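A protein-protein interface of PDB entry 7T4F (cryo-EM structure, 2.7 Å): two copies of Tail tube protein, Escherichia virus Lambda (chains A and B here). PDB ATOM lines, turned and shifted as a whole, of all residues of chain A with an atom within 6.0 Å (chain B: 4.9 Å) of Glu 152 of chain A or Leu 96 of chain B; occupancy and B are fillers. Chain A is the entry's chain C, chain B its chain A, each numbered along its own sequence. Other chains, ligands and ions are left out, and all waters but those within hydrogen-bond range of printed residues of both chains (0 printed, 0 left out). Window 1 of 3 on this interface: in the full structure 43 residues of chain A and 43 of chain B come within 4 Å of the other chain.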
ATOM      1  N   LEU A  49      -8.022  -3.283 -10.734  1.00  0.00           N
ATOM      2  CA  LEU A  49      -8.907  -4.358 -11.164  1.00  0.00           C
ATOM      3  C   LEU A  49      -8.495  -5.656 -10.483  1.00  0.00           C
ATOM      4  O   LEU A  49      -7.373  -6.135 -10.676  1.00  0.00           O
ATOM      5  CB  LEU A  49      -8.865  -4.509 -12.683  1.00  0.00           C
ATOM      6  CG  LEU A  49      -8.932  -3.236 -13.532  1.00  0.00           C
ATOM      7  CD1 LEU A  49      -9.063  -3.589 -15.003  1.00  0.00           C
ATOM      8  CD2 LEU A  49     -10.083  -2.344 -13.096  1.00  0.00           C
ATOM      9  N   ASP A 117      -8.154   6.376 -20.359  1.00  0.00           N
ATOM     10  CA  ASP A 117      -8.849   5.344 -19.598  1.00  0.00           C
ATOM     11  C   ASP A 117     -10.181   5.911 -19.133  1.00  0.00           C
ATOM     12  O   ASP A 117     -10.222   6.988 -18.529  1.00  0.00           O
ATOM     13  CB  ASP A 117      -8.015   4.875 -18.405  1.00  0.00           C
ATOM     14  CG  ASP A 117      -6.936   3.888 -18.800  1.00  0.00           C
ATOM     15  OD1 ASP A 117      -6.776   3.633 -20.011  1.00  0.00           O
ATOM     16  OD2 ASP A 117      -6.247   3.365 -17.898  1.00  0.00           O
ATOM     17  N   MET A 150     -10.339   0.110 -20.917  1.00  0.00           N
ATOM     18  CA  MET A 150      -8.909   0.297 -20.748  1.00  0.00           C
ATOM     19  C   MET A 150      -8.276   0.827 -22.033  1.00  0.00           C
ATOM     20  O   MET A 150      -8.865   0.788 -23.116  1.00  0.00           O
ATOM     21  CB  MET A 150      -8.245  -1.017 -20.335  1.00  0.00           C
ATOM     22  CG  MET A 150      -8.623  -1.503 -18.944  1.00  0.00           C
ATOM     23  SD  MET A 150      -7.537  -0.872 -17.650  1.00  0.00           S
ATOM     24  CE  MET A 150      -8.406   0.615 -17.165  1.00  0.00           C
ATOM     25  N   ALA A 151      -7.049   1.336 -21.896  1.00  0.00           N
ATOM     26  CA  ALA A 151      -6.322   1.839 -23.057  1.00  0.00           C
ATOM     27  C   ALA A 151      -5.953   0.709 -24.009  1.00  0.00           C
ATOM     28  O   ALA A 151      -5.899   0.907 -25.229  1.00  0.00           O
ATOM     29  CB  ALA A 151      -5.070   2.592 -22.607  1.00  0.00           C
ATOM     30  N   GLU A 152      -5.691  -0.484 -23.471  1.00  0.00           N
ATOM     31  CA  GLU A 152      -5.348  -1.625 -24.310  1.00  0.00           C
ATOM     32  C   GLU A 152      -6.521  -2.090 -25.164  1.00  0.00           C
ATOM     33  O   GLU A 152      -6.315  -2.832 -26.129  1.00  0.00           O
ATOM     34  CB  GLU A 152      -4.846  -2.782 -23.444  1.00  0.00           C
ATOM     35  CG  GLU A 152      -3.455  -2.569 -22.869  1.00  0.00           C
ATOM     36  CD  GLU A 152      -3.480  -1.833 -21.543  1.00  0.00           C
ATOM     37  OE1 GLU A 152      -4.524  -1.871 -20.858  1.00  0.00           O
ATOM     38  OE2 GLU A 152      -2.454  -1.217 -21.184  1.00  0.00           O
ATOM     39  N   ASP A 153      -7.744  -1.673 -24.829  1.00  0.00           N
ATOM     40  CA  ASP A 153      -8.905  -2.075 -25.616  1.00  0.00           C
ATOM     41  C   ASP A 153      -8.914  -1.393 -26.978  1.00  0.00           C
ATOM     42  O   ASP A 153      -9.358  -1.980 -27.973  1.00  0.00           O
ATOM     43  CB  ASP A 153     -10.192  -1.761 -24.852  1.00  0.00           C
ATOM     44  CG  ASP A 153     -10.665  -2.925 -24.005  1.00  0.00           C
ATOM     45  OD1 ASP A 153     -11.447  -2.695 -23.059  1.00  0.00           O
ATOM     46  OD2 ASP A 153     -10.255  -4.072 -24.284  1.00  0.00           O
ATOM     47  N   ARG A 154      -8.430  -0.154 -27.045  1.00  0.00           N
ATOM     48  CA  ARG A 154      -8.441   0.629 -28.272  1.00  0.00           C
ATOM     49  C   ARG A 154      -7.162   0.470 -29.085  1.00  0.00           C
ATOM     50  O   ARG A 154      -7.010   1.133 -30.117  1.00  0.00           O
ATOM     51  CB  ARG A 154      -8.673   2.107 -27.949  1.00  0.00           C
ATOM     52  CG  ARG A 154     -10.134   2.524 -27.970  1.00  0.00           C
ATOM     53  CD  ARG A 154     -10.352   3.822 -27.210  1.00  0.00           C
ATOM     54  NE  ARG A 154     -10.857   3.589 -25.863  1.00  0.00           N
ATOM     55  CZ  ARG A 154     -10.118   3.653 -24.764  1.00  0.00           C
ATOM     56  NH1 ARG A 154      -8.829   3.946 -24.814  1.00  0.00           N
ATOM     57  NH2 ARG A 154     -10.688   3.421 -23.585  1.00  0.00           N
ATOM     58  N   SER A 155      -6.280  -0.439 -28.689  1.00  0.00           N
ATOM     59  CA  SER A 155      -4.986  -0.587 -29.396  1.00  0.00           C
ATOM     60  C   SER A 155      -5.188  -1.488 -30.606  1.00  0.00           C
ATOM     61  O   SER A 155      -5.858  -2.523 -30.457  1.00  0.00           O
ATOM     62  CB  SER A 155      -3.919  -1.117 -28.490  1.00  0.00           C
ATOM     63  OG  SER A 155      -3.670  -0.225 -27.416  1.00  0.00           O
ATOM     64  N   TRP B  85       4.679   0.443 -18.163  1.00  0.00           N
ATOM     65  CA  TRP B  85       3.386   0.467 -18.835  1.00  0.00           C
ATOM     66  C   TRP B  85       3.572   0.836 -20.300  1.00  0.00           C
ATOM     67  O   TRP B  85       3.855   1.994 -20.627  1.00  0.00           O
ATOM     68  CB  TRP B  85       2.439   1.448 -18.147  1.00  0.00           C
ATOM     69  CG  TRP B  85       1.108   1.556 -18.823  1.00  0.00           C
ATOM     70  CD1 TRP B  85       0.231   0.540 -19.069  1.00  0.00           C
ATOM     71  CD2 TRP B  85       0.499   2.744 -19.339  1.00  0.00           C
ATOM     72  NE1 TRP B  85      -0.885   1.022 -19.707  1.00  0.00           N
ATOM     73  CE2 TRP B  85      -0.745   2.374 -19.885  1.00  0.00           C
ATOM     74  CE3 TRP B  85       0.886   4.087 -19.394  1.00  0.00           C
ATOM     75  CZ2 TRP B  85      -1.605   3.294 -20.476  1.00  0.00           C
ATOM     76  CZ3 TRP B  85       0.030   4.999 -19.982  1.00  0.00           C
ATOM     77  CH2 TRP B  85      -1.200   4.600 -20.514  1.00  0.00           C
ATOM     78  N   PRO B  87       1.190   0.108 -23.363  1.00  0.00           N
ATOM     79  CA  PRO B  87      -0.027  -0.515 -23.914  1.00  0.00           C
ATOM     80  C   PRO B  87       0.101  -0.930 -25.370  1.00  0.00           C
ATOM     81  O   PRO B  87      -0.655  -1.795 -25.830  1.00  0.00           O
ATOM     82  CB  PRO B  87      -1.089   0.577 -23.723  1.00  0.00           C
ATOM     83  CG  PRO B  87      -0.312   1.851 -23.682  1.00  0.00           C
ATOM     84  CD  PRO B  87       0.970   1.513 -22.983  1.00  0.00           C
ATOM     85  N   GLN B  92       1.556  -6.843 -23.342  1.00  0.00           N
ATOM     86  CA  GLN B  92       0.629  -6.296 -22.356  1.00  0.00           C
ATOM     87  C   GLN B  92      -0.816  -6.416 -22.827  1.00  0.00           C
ATOM     88  O   GLN B  92      -1.725  -6.612 -22.013  1.00  0.00           O
ATOM     89  CB  GLN B  92       0.989  -4.844 -22.046  1.00  0.00           C
ATOM     90  CG  GLN B  92       2.421  -4.667 -21.563  1.00  0.00           C
ATOM     91  CD  GLN B  92       2.600  -3.440 -20.696  1.00  0.00           C
ATOM     92  OE1 GLN B  92       1.626  -2.815 -20.275  1.00  0.00           O
ATOM     93  NE2 GLN B  92       3.849  -3.089 -20.417  1.00  0.00           N
ATOM     94  N   GLN B  93      -1.049  -6.313 -24.138  1.00  0.00           N
ATOM     95  CA  GLN B  93      -2.387  -6.560 -24.666  1.00  0.00           C
ATOM     96  C   GLN B  93      -2.815  -8.002 -24.423  1.00  0.00           C
ATOM     97  O   GLN B  93      -3.959  -8.264 -24.028  1.00  0.00           O
ATOM     98  CB  GLN B  93      -2.431  -6.232 -26.158  1.00  0.00           C
ATOM     99  CG  GLN B  93      -2.140  -4.777 -26.486  1.00  0.00           C
ATOM    100  CD  GLN B  93      -2.213  -4.491 -27.973  1.00  0.00           C
ATOM    101  OE1 GLN B  93      -3.086  -5.003 -28.672  1.00  0.00           O
ATOM    102  NE2 GLN B  93      -1.292  -3.671 -28.464  1.00  0.00           N
ATOM    103  N   ALA B  94      -1.904  -8.953 -24.648  1.00  0.00           N
ATOM    104  CA  ALA B  94      -2.204 -10.350 -24.357  1.00  0.00           C
ATOM    105  C   ALA B  94      -2.423 -10.578 -22.868  1.00  0.00           C
ATOM    106  O   ALA B  94      -3.272 -11.387 -22.487  1.00  0.00           O
ATOM    107  CB  ALA B  94      -1.081 -11.249 -24.874  1.00  0.00           C
ATOM    108  N   LEU B  95      -1.668  -9.881 -22.017  1.00  0.00           N
ATOM    109  CA  LEU B  95      -1.877  -9.982 -20.576  1.00  0.00           C
ATOM    110  C   LEU B  95      -3.259  -9.472 -20.176  1.00  0.00           C
ATOM    111  O   LEU B  95      -3.944 -10.085 -19.347  1.00  0.00           O
ATOM    112  CB  LEU B  95      -0.782  -9.207 -19.846  1.00  0.00           C
ATOM    113  CG  LEU B  95      -0.774  -9.210 -18.320  1.00  0.00           C
ATOM    114  CD1 LEU B  95      -0.536 -10.609 -17.780  1.00  0.00           C
ATOM    115  CD2 LEU B  95       0.295  -8.256 -17.829  1.00  0.00           C
ATOM    116  N   LEU B  96      -3.681  -8.344 -20.751  1.00  0.00           N
ATOM    117  CA  LEU B  96      -5.013  -7.818 -20.464  1.00  0.00           C
ATOM    118  C   LEU B  96      -6.097  -8.769 -20.956  1.00  0.00           C
ATOM    119  O   LEU B  96      -7.110  -8.971 -20.275  1.00  0.00           O
ATOM    120  CB  LEU B  96      -5.181  -6.436 -21.093  1.00  0.00           C
ATOM    121  CG  LEU B  96      -5.049  -5.237 -20.150  1.00  0.00           C
ATOM    122  CD1 LEU B  96      -6.203  -5.197 -19.160  1.00  0.00           C
ATOM    123  CD2 LEU B  96      -3.714  -5.263 -19.420  1.00  0.00           C
ATOM    124  N   ALA B  97      -5.903  -9.362 -22.137  1.00  0.00           N
ATOM    125  CA  ALA B  97      -6.858 -10.349 -22.633  1.00  0.00           C
ATOM    126  C   ALA B  97      -6.903 -11.573 -21.727  1.00  0.00           C
ATOM    127  O   ALA B  97      -7.972 -12.153 -21.506  1.00  0.00           O
ATOM    128  CB  ALA B  97      -6.502 -10.750 -24.065  1.00  0.00           C
ATOM    129  N   TRP B  98      -5.748 -11.986 -21.204  1.00  0.00           N
ATOM    130  CA  TRP B  98      -5.691 -13.100 -20.264  1.00  0.00           C
ATOM    131  C   TRP B  98      -6.474 -12.785 -18.996  1.00  0.00           C
ATOM    132  O   TRP B  98      -7.218 -13.632 -18.488  1.00  0.00           O
ATOM    133  CB  TRP B  98      -4.228 -13.413 -19.941  1.00  0.00           C
ATOM    134  CG  TRP B  98      -3.990 -14.525 -18.960  1.00  0.00           C
ATOM    135  CD1 TRP B  98      -4.876 -15.486 -18.565  1.00  0.00           C
ATOM    136  CD2 TRP B  98      -2.774 -14.784 -18.247  1.00  0.00           C
ATOM    137  NE1 TRP B  98      -4.286 -16.326 -17.652  1.00  0.00           N
ATOM    138  CE2 TRP B  98      -2.996 -15.916 -17.440  1.00  0.00           C
ATOM    139  CE3 TRP B  98      -1.520 -14.167 -18.214  1.00  0.00           C
ATOM    140  CZ2 TRP B  98      -2.009 -16.445 -16.610  1.00  0.00           C
ATOM    141  CZ3 TRP B  98      -0.543 -14.693 -17.390  1.00  0.00           C
ATOM    142  CH2 TRP B  98      -0.793 -15.820 -16.599  1.00  0.00           C
ATOM    143  N   PHE B  99      -6.319 -11.569 -18.471  1.00  0.00           N
ATOM    144  CA  PHE B  99      -7.080 -11.180 -17.285  1.00  0.00           C
ATOM    145  C   PHE B  99      -8.576 -11.139 -17.574  1.00  0.00           C
ATOM    146  O   PHE B  99      -9.386 -11.580 -16.750  1.00  0.00           O
ATOM    147  CB  PHE B  99      -6.603  -9.824 -16.765  1.00  0.00           C
ATOM    148  CG  PHE B  99      -7.437  -9.285 -15.635  1.00  0.00           C
ATOM    149  CD1 PHE B  99      -7.290  -9.782 -14.351  1.00  0.00           C
ATOM    150  CD2 PHE B  99      -8.368  -8.284 -15.857  1.00  0.00           C
ATOM    151  CE1 PHE B  99      -8.056  -9.291 -13.310  1.00  0.00           C
ATOM    152  CE2 PHE B  99      -9.137  -7.790 -14.820  1.00  0.00           C
ATOM    153  CZ  PHE B  99      -8.980  -8.294 -13.545  1.00  0.00           C
ATOM    154  N   ASN B 100      -8.962 -10.606 -18.736  1.00  0.00           N
ATOM    155  CA  ASN B 100     -10.381 -10.479 -19.055  1.00  0.00           C
ATOM    156  C   ASN B 100     -11.031 -11.840 -19.285  1.00  0.00           C
ATOM    157  O   ASN B 100     -12.173 -12.066 -18.869  1.00  0.00           O
ATOM    158  CB  ASN B 100     -10.564  -9.584 -20.282  1.00  0.00           C
ATOM    159  CG  ASN B 100     -10.409  -8.112 -19.957  1.00  0.00           C
ATOM    160  OD1 ASN B 100     -10.788  -7.658 -18.877  1.00  0.00           O
ATOM    161  ND2 ASN B 100      -9.852  -7.355 -20.895  1.00  0.00           N
ATOM    162  N   ILE B 126      -4.703  -6.231 -11.410  1.00  0.00           N
ATOM    163  CA  ILE B 126      -4.073  -5.339 -12.377  1.00  0.00           C
ATOM    164  C   ILE B 126      -4.072  -3.939 -11.777  1.00  0.00           C
ATOM    165  O   ILE B 126      -5.134  -3.419 -11.414  1.00  0.00           O
ATOM    166  CB  ILE B 126      -4.800  -5.350 -13.733  1.00  0.00           C
ATOM    167  CG1 ILE B 126      -4.490  -6.643 -14.495  1.00  0.00           C
ATOM    168  CG2 ILE B 126      -4.425  -4.127 -14.555  1.00  0.00           C
ATOM    169  CD1 ILE B 126      -3.201  -6.601 -15.287  1.00  0.00           C
ATOM    170  N   ARG B 138       3.004  -0.836 -14.376  1.00  0.00           N
ATOM    171  CA  ARG B 138       1.874  -1.755 -14.415  1.00  0.00           C
ATOM    172  C   ARG B 138       2.166  -2.907 -13.462  1.00  0.00           C
ATOM    173  O   ARG B 138       3.167  -3.611 -13.627  1.00  0.00           O
ATOM    174  CB  ARG B 138       1.646  -2.270 -15.837  1.00  0.00           C
ATOM    175  CG  ARG B 138       0.684  -3.441 -15.945  1.00  0.00           C
ATOM    176  CD  ARG B 138      -0.727  -3.037 -15.559  1.00  0.00           C
ATOM    177  NE  ARG B 138      -1.490  -2.563 -16.707  1.00  0.00           N
ATOM    178  CZ  ARG B 138      -2.521  -1.734 -16.631  1.00  0.00           C
ATOM    179  NH1 ARG B 138      -2.939  -1.254 -15.471  1.00  0.00           N
ATOM    180  NH2 ARG B 138      -3.149  -1.375 -17.748  1.00  0.00           N
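The backbone carbonyl oxygen (O) of Leu 49 of chain A lies within hydrogen-bond range of the backbone NH (N) of Ile 126 of chain B. The indole nitrogen (NE1) of Trp 85 of chain B sits at hydrogen-bond distance from the side-chain carboxylate (OE2) of Glu 152 of chain A, at 3.1 Å. The guanidinium group (NH2) of Arg 138 of chain B is in salt-bridge range of the side-chain carboxylate (OE1) of Glu 152 of chain A (3.4 Å).
The side-chain hydroxyl of Ser 155 of chain A sits at hydrogen-bond distance from the backbone carbonyl oxygen of Ala 151 of chain A (3.3 Å). NE2 of Gln 93 of chain B lies within hydrogen-bond range of O of Pro 87 of chain B, at 3.3 Å. The side-chain amide nitrogen of Asn 100 of chain B is in hydrogen-bond range of the backbone carbonyl oxygen of Leu 96 of chain B.
Leu 49 of chain A touches Phe 99 of chain B (CB to CZ, 3.9 Å). Pro 87 of chain B touches Glu 152 of chain A. CG of Leu 96 of chain B touches OE1 of Glu 152 of chain A, 3.5 Å away. Ser 155 of chain A touches Pro 87 of chain B. Ser 155 of chain A touches Gln 93 of chain B.
Ala 151 of chain A touches none of the printed residues of chain B. Of chain B, only Trp 85, Pro 87, Leu 96 and Arg 138 come within 4 Å of Glu 152 of chain A. Of the printed residues of chain A, Pro 87 of chain B touches Glu 152 and Ser 155. Of the printed residues of chain A, Gln 93 of chain B touches Ser 155 (3.7 Å). Leu 96 of chain B touches just one residue of chain A: Glu 152. Printed residues of chain A within 4 Å of Phe 99 of chain B: Leu 49. Printed residues of chain A within 4 Å of Ile 126 of chain B: Leu 49 (2.8 Å). Printed residues of chain A within 4 Å of Arg 138 of chain B: Glu 152. The nearest residue of chain B that does not touch Glu 152 of chain A is Gln 93 of chain B (4.4 Å).
Of the 8 printed residues of chain A, 3 touch a printed residue of chain B. Hydrophobic or aromatic side chains of chain A that line the printed part of chain B: Leu 49. Hydrophobic or aromatic side chains of chain B that line the printed part of chain A: Trp 85, Pro 87, Leu 96 and Phe 99.
No position is printed for both chains. Of the 8 pairs that touch across the chains among the printed residues, none has its exchanged pair printed and touching as well.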
